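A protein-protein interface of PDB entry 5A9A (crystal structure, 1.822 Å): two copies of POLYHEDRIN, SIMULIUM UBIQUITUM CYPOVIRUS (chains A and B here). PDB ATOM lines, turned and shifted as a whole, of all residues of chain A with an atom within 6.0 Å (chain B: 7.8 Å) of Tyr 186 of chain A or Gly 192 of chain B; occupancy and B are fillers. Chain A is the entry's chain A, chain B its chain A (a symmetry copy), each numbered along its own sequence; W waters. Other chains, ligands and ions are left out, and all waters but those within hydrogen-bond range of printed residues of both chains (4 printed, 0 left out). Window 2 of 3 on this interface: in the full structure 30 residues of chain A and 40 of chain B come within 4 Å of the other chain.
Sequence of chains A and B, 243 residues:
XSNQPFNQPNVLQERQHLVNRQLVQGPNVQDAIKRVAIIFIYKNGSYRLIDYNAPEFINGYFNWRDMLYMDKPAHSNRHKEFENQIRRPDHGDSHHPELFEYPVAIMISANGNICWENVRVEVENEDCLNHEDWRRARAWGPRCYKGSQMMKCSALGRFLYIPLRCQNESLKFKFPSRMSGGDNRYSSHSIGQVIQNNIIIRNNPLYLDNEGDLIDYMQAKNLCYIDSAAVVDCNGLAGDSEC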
ATOM      1  N   GLU A  56      -3.794  17.244   0.673  1.00  0.00           N
ATOM      2  CA  GLU A  56      -4.573  17.311  -0.565  1.00  0.00           C
ATOM      3  C   GLU A  56      -5.117  15.939  -0.975  1.00  0.00           C
ATOM      4  O   GLU A  56      -6.318  15.776  -1.183  1.00  0.00           O
ATOM      5  CB  GLU A  56      -3.745  17.907  -1.706  1.00  0.00           C
ATOM      6  CG  GLU A  56      -2.880  19.092  -1.309  1.00  0.00           C
ATOM      7  CD  GLU A  56      -3.659  20.176  -0.588  1.00  0.00           C
ATOM      8  OE1 GLU A  56      -4.890  20.273  -0.786  1.00  0.00           O
ATOM      9  OE2 GLU A  56      -3.035  20.933   0.183  1.00  0.00           O
ATOM     10  N   PHE A  57      -4.233  14.957  -1.103  1.00  0.00           N
ATOM     11  CA  PHE A  57      -4.658  13.594  -1.417  1.00  0.00           C
ATOM     12  C   PHE A  57      -3.597  12.573  -1.042  1.00  0.00           C
ATOM     13  O   PHE A  57      -2.403  12.825  -1.187  1.00  0.00           O
ATOM     14  CB  PHE A  57      -5.016  13.453  -2.905  1.00  0.00           C
ATOM     15  CG  PHE A  57      -3.901  13.815  -3.841  1.00  0.00           C
ATOM     16  CD1 PHE A  57      -2.981  12.862  -4.249  1.00  0.00           C
ATOM     17  CD2 PHE A  57      -3.782  15.106  -4.331  1.00  0.00           C
ATOM     18  CE1 PHE A  57      -1.953  13.195  -5.118  1.00  0.00           C
ATOM     19  CE2 PHE A  57      -2.761  15.444  -5.201  1.00  0.00           C
ATOM     20  CZ  PHE A  57      -1.845  14.489  -5.595  1.00  0.00           C
ATOM     21  N   MET A 179     -13.360  19.293  -1.840  1.00  0.00           N
ATOM     22  CA  MET A 179     -13.150  20.726  -1.977  1.00  0.00           C
ATOM     23  C   MET A 179     -14.115  21.475  -1.073  1.00  0.00           C
ATOM     24  O   MET A 179     -15.037  20.886  -0.508  1.00  0.00           O
ATOM     25  CB  MET A 179     -13.368  21.162  -3.424  1.00  0.00           C
ATOM     26  CG  MET A 179     -12.317  20.637  -4.383  1.00  0.00           C
ATOM     27  SD  MET A 179     -10.661  21.167  -3.910  1.00  0.00           S
ATOM     28  CE  MET A 179      -9.662  20.131  -4.973  1.00  0.00           C
ATOM     29  N   ASP A 183     -15.616  25.032  -5.076  1.00  0.00           N
ATOM     30  CA  ASP A 183     -14.335  25.658  -5.383  1.00  0.00           C
ATOM     31  C   ASP A 183     -13.281  24.607  -5.702  1.00  0.00           C
ATOM     32  O   ASP A 183     -12.673  24.031  -4.801  1.00  0.00           O
ATOM     33  CB  ASP A 183     -13.851  26.527  -4.225  1.00  0.00           C
ATOM     34  CG  ASP A 183     -12.578  27.289  -4.562  1.00  0.00           C
ATOM     35  OD1 ASP A 183     -11.994  27.035  -5.637  1.00  0.00           O
ATOM     36  OD2 ASP A 183     -12.154  28.145  -3.757  1.00  0.00           O
ATOM     37  N   ASN A 184     -13.065  24.367  -6.988  1.00  0.00           N
ATOM     38  CA  ASN A 184     -12.035  23.436  -7.425  1.00  0.00           C
ATOM     39  C   ASN A 184     -10.658  24.059  -7.259  1.00  0.00           C
ATOM     40  O   ASN A 184     -10.296  24.979  -7.990  1.00  0.00           O
ATOM     41  CB  ASN A 184     -12.253  23.057  -8.887  1.00  0.00           C
ATOM     42  CG  ASN A 184     -11.256  22.031  -9.375  1.00  0.00           C
ATOM     43  OD1 ASN A 184     -10.509  21.451  -8.586  1.00  0.00           O
ATOM     44  ND2 ASN A 184     -11.243  21.793 -10.683  1.00  0.00           N
ATOM     45  N   ARG A 185      -9.889  23.558  -6.297  1.00  0.00           N
ATOM     46  CA  ARG A 185      -8.564  24.110  -6.032  1.00  0.00           C
ATOM     47  C   ARG A 185      -7.537  23.668  -7.073  1.00  0.00           C
ATOM     48  O   ARG A 185      -6.367  24.036  -6.998  1.00  0.00           O
ATOM     49  CB  ARG A 185      -8.100  23.750  -4.621  1.00  0.00           C
ATOM     50  CG  ARG A 185      -8.734  24.630  -3.552  1.00  0.00           C
ATOM     51  CD  ARG A 185      -8.366  24.176  -2.153  1.00  0.00           C
ATOM     52  NE  ARG A 185      -6.956  24.400  -1.849  1.00  0.00           N
ATOM     53  CZ  ARG A 185      -6.310  23.815  -0.844  1.00  0.00           C
ATOM     54  NH1 ARG A 185      -6.941  22.952  -0.056  1.00  0.00           N
ATOM     55  NH2 ARG A 185      -5.025  24.079  -0.636  1.00  0.00           N
ATOM     56  N   TYR A 186      -7.982  22.887  -8.051  1.00  0.00           N
ATOM     57  CA  TYR A 186      -7.144  22.580  -9.203  1.00  0.00           C
ATOM     58  C   TYR A 186      -7.340  23.639 -10.276  1.00  0.00           C
ATOM     59  O   TYR A 186      -6.863  23.500 -11.401  1.00  0.00           O
ATOM     60  CB  TYR A 186      -7.430  21.173  -9.717  1.00  0.00           C
ATOM     61  CG  TYR A 186      -6.921  20.144  -8.748  1.00  0.00           C
ATOM     62  CD1 TYR A 186      -5.571  19.829  -8.700  1.00  0.00           C
ATOM     63  CD2 TYR A 186      -7.776  19.520  -7.848  1.00  0.00           C
ATOM     64  CE1 TYR A 186      -5.086  18.907  -7.801  1.00  0.00           C
ATOM     65  CE2 TYR A 186      -7.300  18.590  -6.946  1.00  0.00           C
ATOM     66  CZ  TYR A 186      -5.953  18.293  -6.925  1.00  0.00           C
ATOM     67  OH  TYR A 186      -5.474  17.371  -6.027  1.00  0.00           O
ATOM     68  N   SER A 187      -8.052  24.698  -9.902  1.00  0.00           N
ATOM     69  CA  SER A 187      -8.119  25.914 -10.698  1.00  0.00           C
ATOM     70  C   SER A 187      -6.776  26.629 -10.625  1.00  0.00           C
ATOM     71  O   SER A 187      -5.958  26.337  -9.753  1.00  0.00           O
ATOM     72  CB  SER A 187      -9.227  26.826 -10.167  1.00  0.00           C
ATOM     73  OG  SER A 187     -10.499  26.231 -10.346  1.00  0.00           O
ATOM     74  N   SER A 188      -6.553  27.568 -11.539  1.00  0.00           N
ATOM     75  CA  SER A 188      -5.269  28.261 -11.635  1.00  0.00           C
ATOM     76  C   SER A 188      -4.935  29.084 -10.388  1.00  0.00           C
ATOM     77  O   SER A 188      -3.762  29.326 -10.103  1.00  0.00           O
ATOM     78  CB  SER A 188      -5.252  29.165 -12.871  1.00  0.00           C
ATOM     79  OG  SER A 188      -5.496  28.416 -14.049  1.00  0.00           O
ATOM     80  N   SER A 190      -5.381  28.240  -7.264  1.00  0.00           N
ATOM     81  CA  SER A 190      -5.123  27.467  -6.055  1.00  0.00           C
ATOM     82  C   SER A 190      -4.217  26.258  -6.262  1.00  0.00           C
ATOM     83  O   SER A 190      -3.724  25.676  -5.295  1.00  0.00           O
ATOM     84  CB  SER A 190      -6.461  26.988  -5.484  1.00  0.00           C
ATOM     85  OG  SER A 190      -7.332  28.077  -5.237  1.00  0.00           O
ATOM     86  N   ILE A 191      -3.996  25.881  -7.516  1.00  0.00           N
ATOM     87  CA  ILE A 191      -3.389  24.590  -7.821  1.00  0.00           C
ATOM     88  C   ILE A 191      -1.907  24.510  -7.445  1.00  0.00           C
ATOM     89  O   ILE A 191      -1.438  23.465  -6.996  1.00  0.00           O
ATOM     90  CB  ILE A 191      -3.591  24.211  -9.304  1.00  0.00           C
ATOM     91  CG1 ILE A 191      -3.174  22.757  -9.539  1.00  0.00           C
ATOM     92  CG2 ILE A 191      -2.832  25.167 -10.219  1.00  0.00           C
ATOM     93  CD1 ILE A 191      -3.501  22.255 -10.923  1.00  0.00           C
ATOM     94  N   VAL A 194      -1.789  23.495  -3.903  1.00  0.00           N
ATOM     95  CA  VAL A 194      -2.204  22.106  -3.736  1.00  0.00           C
ATOM     96  C   VAL A 194      -1.050  21.162  -4.076  1.00  0.00           C
ATOM     97  O   VAL A 194      -0.735  20.253  -3.308  1.00  0.00           O
ATOM     98  CB  VAL A 194      -3.419  21.762  -4.619  1.00  0.00           C
ATOM     99  CG1 VAL A 194      -3.674  20.256  -4.617  1.00  0.00           C
ATOM    100  CG2 VAL A 194      -4.656  22.510  -4.144  1.00  0.00           C
ATOM    101  N   ILE A 195      -0.417  21.391  -5.222  1.00  0.00           N
ATOM    102  CA  ILE A 195       0.668  20.531  -5.686  1.00  0.00           C
ATOM    103  C   ILE A 195       1.860  20.551  -4.731  1.00  0.00           C
ATOM    104  O   ILE A 195       2.392  19.499  -4.376  1.00  0.00           O
ATOM    105  CB  ILE A 195       1.143  20.944  -7.090  1.00  0.00           C
ATOM    106  CG1 ILE A 195       0.060  20.629  -8.123  1.00  0.00           C
ATOM    107  CG2 ILE A 195       2.436  20.222  -7.448  1.00  0.00           C
ATOM    108  CD1 ILE A 195       0.273  21.298  -9.464  1.00  0.00           C
ATOM    109  N   ARG B 185      -5.126  18.006 -21.083  1.00  0.00           N
ATOM    110  CA  ARG B 185      -5.736  17.596 -19.822  1.00  0.00           C
ATOM    111  C   ARG B 185      -5.088  18.281 -18.620  1.00  0.00           C
ATOM    112  O   ARG B 185      -5.476  18.046 -17.478  1.00  0.00           O
ATOM    113  CB  ARG B 185      -5.697  16.076 -19.671  1.00  0.00           C
ATOM    114  CG  ARG B 185      -6.782  15.378 -20.478  1.00  0.00           C
ATOM    115  CD  ARG B 185      -6.649  13.868 -20.421  1.00  0.00           C
ATOM    116  NE  ARG B 185      -6.948  13.333 -19.097  1.00  0.00           N
ATOM    117  CZ  ARG B 185      -6.603  12.114 -18.692  1.00  0.00           C
ATOM    118  NH1 ARG B 185      -5.926  11.308 -19.502  1.00  0.00           N
ATOM    119  NH2 ARG B 185      -6.919  11.706 -17.468  1.00  0.00           N
ATOM    120  N   TYR B 186      -4.108  19.138 -18.882  1.00  0.00           N
ATOM    121  CA  TYR B 186      -3.566  19.997 -17.837  1.00  0.00           C
ATOM    122  C   TYR B 186      -4.363  21.290 -17.771  1.00  0.00           C
ATOM    123  O   TYR B 186      -3.987  22.234 -17.079  1.00  0.00           O
ATOM    124  CB  TYR B 186      -2.077  20.244 -18.061  1.00  0.00           C
ATOM    125  CG  TYR B 186      -1.291  18.992 -17.798  1.00  0.00           C
ATOM    126  CD1 TYR B 186      -1.007  18.598 -16.499  1.00  0.00           C
ATOM    127  CD2 TYR B 186      -0.869  18.177 -18.842  1.00  0.00           C
ATOM    128  CE1 TYR B 186      -0.308  17.440 -16.242  1.00  0.00           C
ATOM    129  CE2 TYR B 186      -0.163  17.017 -18.595  1.00  0.00           C
ATOM    130  CZ  TYR B 186       0.108  16.653 -17.292  1.00  0.00           C
ATOM    131  OH  TYR B 186       0.808  15.497 -17.040  1.00  0.00           O
ATOM    132  N   SER B 187      -5.472  21.309 -18.507  1.00  0.00           N
ATOM    133  CA  SER B 187      -6.484  22.345 -18.365  1.00  0.00           C
ATOM    134  C   SER B 187      -7.211  22.150 -17.041  1.00  0.00           C
ATOM    135  O   SER B 187      -7.125  21.084 -16.431  1.00  0.00           O
ATOM    136  CB  SER B 187      -7.478  22.264 -19.526  1.00  0.00           C
ATOM    137  OG  SER B 187      -6.845  22.572 -20.755  1.00  0.00           O
ATOM    138  N   SER B 188      -7.930  23.178 -16.603  1.00  0.00           N
ATOM    139  CA  SER B 188      -8.599  23.152 -15.302  1.00  0.00           C
ATOM    140  C   SER B 188      -9.677  22.069 -15.202  1.00  0.00           C
ATOM    141  O   SER B 188      -9.988  21.605 -14.105  1.00  0.00           O
ATOM    142  CB  SER B 188      -9.212  24.522 -15.000  1.00  0.00           C
ATOM    143  OG  SER B 188      -8.221  25.536 -15.024  1.00  0.00           O
ATOM    144  N   HIS B 189     -10.249  21.675 -16.336  1.00  0.00           N
ATOM    145  CA  HIS B 189     -11.300  20.656 -16.345  1.00  0.00           C
ATOM    146  C   HIS B 189     -10.775  19.282 -15.943  1.00  0.00           C
ATOM    147  O   HIS B 189     -11.485  18.491 -15.320  1.00  0.00           O
ATOM    148  CB  HIS B 189     -11.921  20.530 -17.740  1.00  0.00           C
ATOM    149  CG  HIS B 189     -12.812  21.673 -18.116  1.00  0.00           C
ATOM    150  ND1 HIS B 189     -13.396  22.499 -17.181  1.00  0.00           N
ATOM    151  CD2 HIS B 189     -13.222  22.123 -19.325  1.00  0.00           C
ATOM    152  CE1 HIS B 189     -14.125  23.411 -17.798  1.00  0.00           C
ATOM    153  NE2 HIS B 189     -14.040  23.204 -19.100  1.00  0.00           N
ATOM    154  N   SER B 190      -9.531  18.999 -16.309  1.00  0.00           N
ATOM    155  CA  SER B 190      -9.043  17.626 -16.333  1.00  0.00           C
ATOM    156  C   SER B 190      -7.827  17.375 -15.447  1.00  0.00           C
ATOM    157  O   SER B 190      -7.475  16.224 -15.183  1.00  0.00           O
ATOM    158  CB  SER B 190      -8.686  17.256 -17.775  1.00  0.00           C
ATOM    159  OG  SER B 190      -9.794  17.436 -18.639  1.00  0.00           O
ATOM    160  N   ILE B 191      -7.188  18.444 -14.986  1.00  0.00           N
ATOM    161  CA  ILE B 191      -5.867  18.330 -14.376  1.00  0.00           C
ATOM    162  C   ILE B 191      -5.886  17.646 -13.006  1.00  0.00           C
ATOM    163  O   ILE B 191      -4.970  16.896 -12.677  1.00  0.00           O
ATOM    164  CB  ILE B 191      -5.172  19.706 -14.283  1.00  0.00           C
ATOM    165  CG1 ILE B 191      -3.706  19.531 -13.879  1.00  0.00           C
ATOM    166  CG2 ILE B 191      -5.914  20.627 -13.319  1.00  0.00           C
ATOM    167  CD1 ILE B 191      -2.911  20.811 -13.932  1.00  0.00           C
ATOM    168  N   GLY B 192      -6.924  17.894 -12.215  1.00  0.00           N
ATOM    169  CA  GLY B 192      -7.058  17.231 -10.929  1.00  0.00           C
ATOM    170  C   GLY B 192      -6.956  15.720 -11.076  1.00  0.00           C
ATOM    171  O   GLY B 192      -6.237  15.046 -10.336  1.00  0.00           O
ATOM    172  N   GLN B 193      -7.678  15.188 -12.054  1.00  0.00           N
ATOM    173  CA  GLN B 193      -7.686  13.754 -12.315  1.00  0.00           C
ATOM    174  C   GLN B 193      -6.317  13.257 -12.784  1.00  0.00           C
ATOM    175  O   GLN B 193      -5.858  12.195 -12.368  1.00  0.00           O
ATOM    176  CB  GLN B 193      -8.752  13.420 -13.358  1.00  0.00           C
ATOM    177  CG  GLN B 193      -8.700  11.989 -13.869  1.00  0.00           C
ATOM    178  CD  GLN B 193      -9.804  11.696 -14.863  1.00  0.00           C
ATOM    179  OE1 GLN B 193     -10.855  12.339 -14.845  1.00  0.00           O
ATOM    180  NE2 GLN B 193      -9.568  10.728 -15.744  1.00  0.00           N
ATOM    181  N   VAL B 194      -5.669  14.024 -13.653  1.00  0.00           N
ATOM    182  CA  VAL B 194      -4.346  13.652 -14.143  1.00  0.00           C
ATOM    183  C   VAL B 194      -3.363  13.532 -12.979  1.00  0.00           C
ATOM    184  O   VAL B 194      -2.647  12.539 -12.860  1.00  0.00           O
ATOM    185  CB  VAL B 194      -3.805  14.673 -15.163  1.00  0.00           C
ATOM    186  CG1 VAL B 194      -2.334  14.400 -15.466  1.00  0.00           C
ATOM    187  CG2 VAL B 194      -4.627  14.637 -16.444  1.00  0.00           C
ATOM    188  N   ILE B 195      -3.343  14.544 -12.116  1.00  0.00           N
ATOM    189  CA  ILE B 195      -2.414  14.576 -10.991  1.00  0.00           C
ATOM    190  C   ILE B 195      -2.654  13.421 -10.019  1.00  0.00           C
ATOM    191  O   ILE B 195      -1.710  12.745  -9.610  1.00  0.00           O
ATOM    192  CB  ILE B 195      -2.515  15.906 -10.223  1.00  0.00           C
ATOM    193  CG1 ILE B 195      -1.971  17.049 -11.081  1.00  0.00           C
ATOM    194  CG2 ILE B 195      -1.746  15.823  -8.911  1.00  0.00           C
ATOM    195  CD1 ILE B 195      -2.334  18.428 -10.574  1.00  0.00           C
ATOM    196  N   GLN B 196      -3.914  13.195  -9.659  1.00  0.00           N
ATOM    197  CA  GLN B 196      -4.249  12.195  -8.653  1.00  0.00           C
ATOM    198  C   GLN B 196      -4.189  10.776  -9.211  1.00  0.00           C
ATOM    199  O   GLN B 196      -4.013   9.820  -8.460  1.00  0.00           O
ATOM    200  CB  GLN B 196      -5.636  12.475  -8.072  1.00  0.00           C
ATOM    201  CG  GLN B 196      -5.720  13.776  -7.294  1.00  0.00           C
ATOM    202  CD  GLN B 196      -7.081  13.996  -6.665  1.00  0.00           C
ATOM    203  OE1 GLN B 196      -8.069  13.386  -7.065  1.00  0.00           O
ATOM    204  NE2 GLN B 196      -7.137  14.866  -5.666  1.00  0.00           N
ATOM    205  N   ASN B 197      -4.334  10.638 -10.525  1.00  0.00           N
ATOM    206  CA  ASN B 197      -4.266   9.325 -11.161  1.00  0.00           C
ATOM    207  C   ASN B 197      -2.839   8.879 -11.447  1.00  0.00           C
ATOM    208  O   ASN B 197      -2.578   7.686 -11.602  1.00  0.00           O
ATOM    209  CB  ASN B 197      -5.062   9.313 -12.468  1.00  0.00           C
ATOM    210  CG  ASN B 197      -6.514   8.926 -12.267  1.00  0.00           C
ATOM    211  OD1 ASN B 197      -6.988   8.801 -11.138  1.00  0.00           O
ATOM    212  ND2 ASN B 197      -7.229   8.732 -13.368  1.00  0.00           N
ATOM    213  N   ASN B 198      -1.910   9.826 -11.529  1.00  0.00           N
ATOM    214  CA  ASN B 198      -0.550   9.473 -11.908  1.00  0.00           C
ATOM    215  C   ASN B 198       0.246   8.943 -10.724  1.00  0.00           C
ATOM    216  O   ASN B 198       1.068   9.642 -10.134  1.00  0.00           O
ATOM    217  CB  ASN B 198       0.175  10.638 -12.583  1.00  0.00           C
ATOM    218  CG  ASN B 198       1.274  10.162 -13.511  1.00  0.00           C
ATOM    219  OD1 ASN B 198       1.012   9.411 -14.454  1.00  0.00           O
ATOM    220  ND2 ASN B 198       2.510  10.582 -13.249  1.00  0.00           N
HETATM  221  O   HOH W   1      -8.669  27.977 -13.716  1.00  0.00           O
HETATM  222  O   HOH W   2      -9.164  19.681 -12.226  1.00  0.00           O
HETATM  223  O   HOH W   3      -5.955  24.808 -13.604  1.00  0.00           O
HETATM  224  O   HOH W   4      -7.015  17.515  -3.679  1.00  0.00           O
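Tyr 186 of chain A touches Ile 191 of chain B, but with the chains exchanged Ile 191 of chain A does not touch Tyr 186 of chain B (6.2 Å). Tyr 186 of chain A touches Ile 195 of chain B, but with the chains exchanged Ile 195 of chain A does not touch Tyr 186 of chain B (7.6 Å). Ile 191 of chain B touches its own counterpart, Ile 191 of chain A. 8 positions are printed for both chains. Of the 8 pairs that touch across the chains among the printed residues, 1 has its exchanged pair printed and touching as well.
The side-chain amide oxygen (OD1) of Asn 184 of chain A sits at hydrogen-bond distance from the backbone NH (N) of Tyr 186 of chain A, at 3.0 Å. The side-chain hydroxyl of Ser 187 of chain A is in hydrogen-bond range of the backbone carbonyl oxygen of Asn 184 of chain A. The backbone NH (N) of Ile 191 of chain A is in hydrogen-bond range of the backbone carbonyl oxygen (O) of Arg 185 of chain A. The backbone carbonyl oxygen (O) of Arg 185 of chain B sits at hydrogen-bond distance from the backbone NH (N) of Ile 191 of chain B (3.0 Å).
Of the 14 printed residues of chain B, 5 touch a printed residue of chain A. Printed residues of chain B that touch a printed residue of chain A: Ser 188, Ile 191, Gly 192, Ile 195 and Gln 196. Hydrophobic or aromatic side chains of chain B that line the printed part of chain A: Ile 191 and Ile 195. Along chain B the printed residues that touch a printed residue of chain A span positions 188 to 196. Of the 13 printed residues of chain A, 4 touch a printed residue of chain B. Hydrophobic or aromatic side chains of chain A within 4 Å of the printed part of chain B: Phe 57, Tyr 186 and Ile 191. Among the printed residues, 8 pairs touch across the chains.
Phe 57 of chain A touches Ile 195 of chain B (CZ to CG2, 3.6 Å). Phe 57 of chain A touches Gln 196 of chain B. ND2 of Asn 184 of chain A touches O of Ser 188 of chain B, 3.6 Å away. Tyr 186 of chain A touches Ile 191 of chain B. Tyr 186 of chain A touches Gly 192 of chain B (CG to CA, 3.6 Å). CD1 of Ile 195 of chain B touches CE1 of Tyr 186 of chain A, at 3.9 Å. Ile 191 of chain A touches Ile 191 of chain B (CD1 to CD1, 3.4 Å).
The side-chain hydroxyl of Tyr 186 of chain A is in hydrogen-bond range of the side-chain amide nitrogen of Gln 196 of chain B (3.0 Å).
Water W3 lies within hydrogen-bond range of the backbone carbonyl oxygen of Tyr 186 of chain A, the side-chain hydroxyl of Ser 188 of chain B and the backbone NH of Ser 188 of chain A. Water W1 bridges the side-chain hydroxyl of Ser 188 of chain B (2.8 Å) and the backbone NH of Ser 188 of chain A (3.1 Å). Water W4 lies within hydrogen-bond range of the side-chain hydroxyl (OH) of Tyr 186 of chain A, the backbone carbonyl oxygen (O) of Glu 56 of chain A and the side-chain amide nitrogen (NE2) of Gln 196 of chain B. Water W2 lies within hydrogen-bond range of the backbone carbonyl oxygen (O) of Ser 188 of chain B, the backbone NH (N) of Gly 192 of chain B and the side-chain amide nitrogen (ND2) of Asn 184 of chain A.
Printed residues of chain B within 4 Å of Asn 184 of chain A: Ser 188 (3.6 Å). Tyr 186 of chain A touches four residues of chain B. Of the printed residues of chain B, Ile 191 of chain A touches Ile 191. Printed residues of chain A within 4 Å of Ser 188 of chain B: Asn 184. Of the printed residues of chain A, Ile 191 of chain B touches Tyr 186 (3.6 Å) and Ile 191 (3.4 Å). Gly 192 of chain B touches just one residue of chain A: Tyr 186 (3.6 Å). Of the printed residues of chain A, Gln 196 of chain B touches Phe 57 (3.6 Å) and Tyr 186 (3.0 Å).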
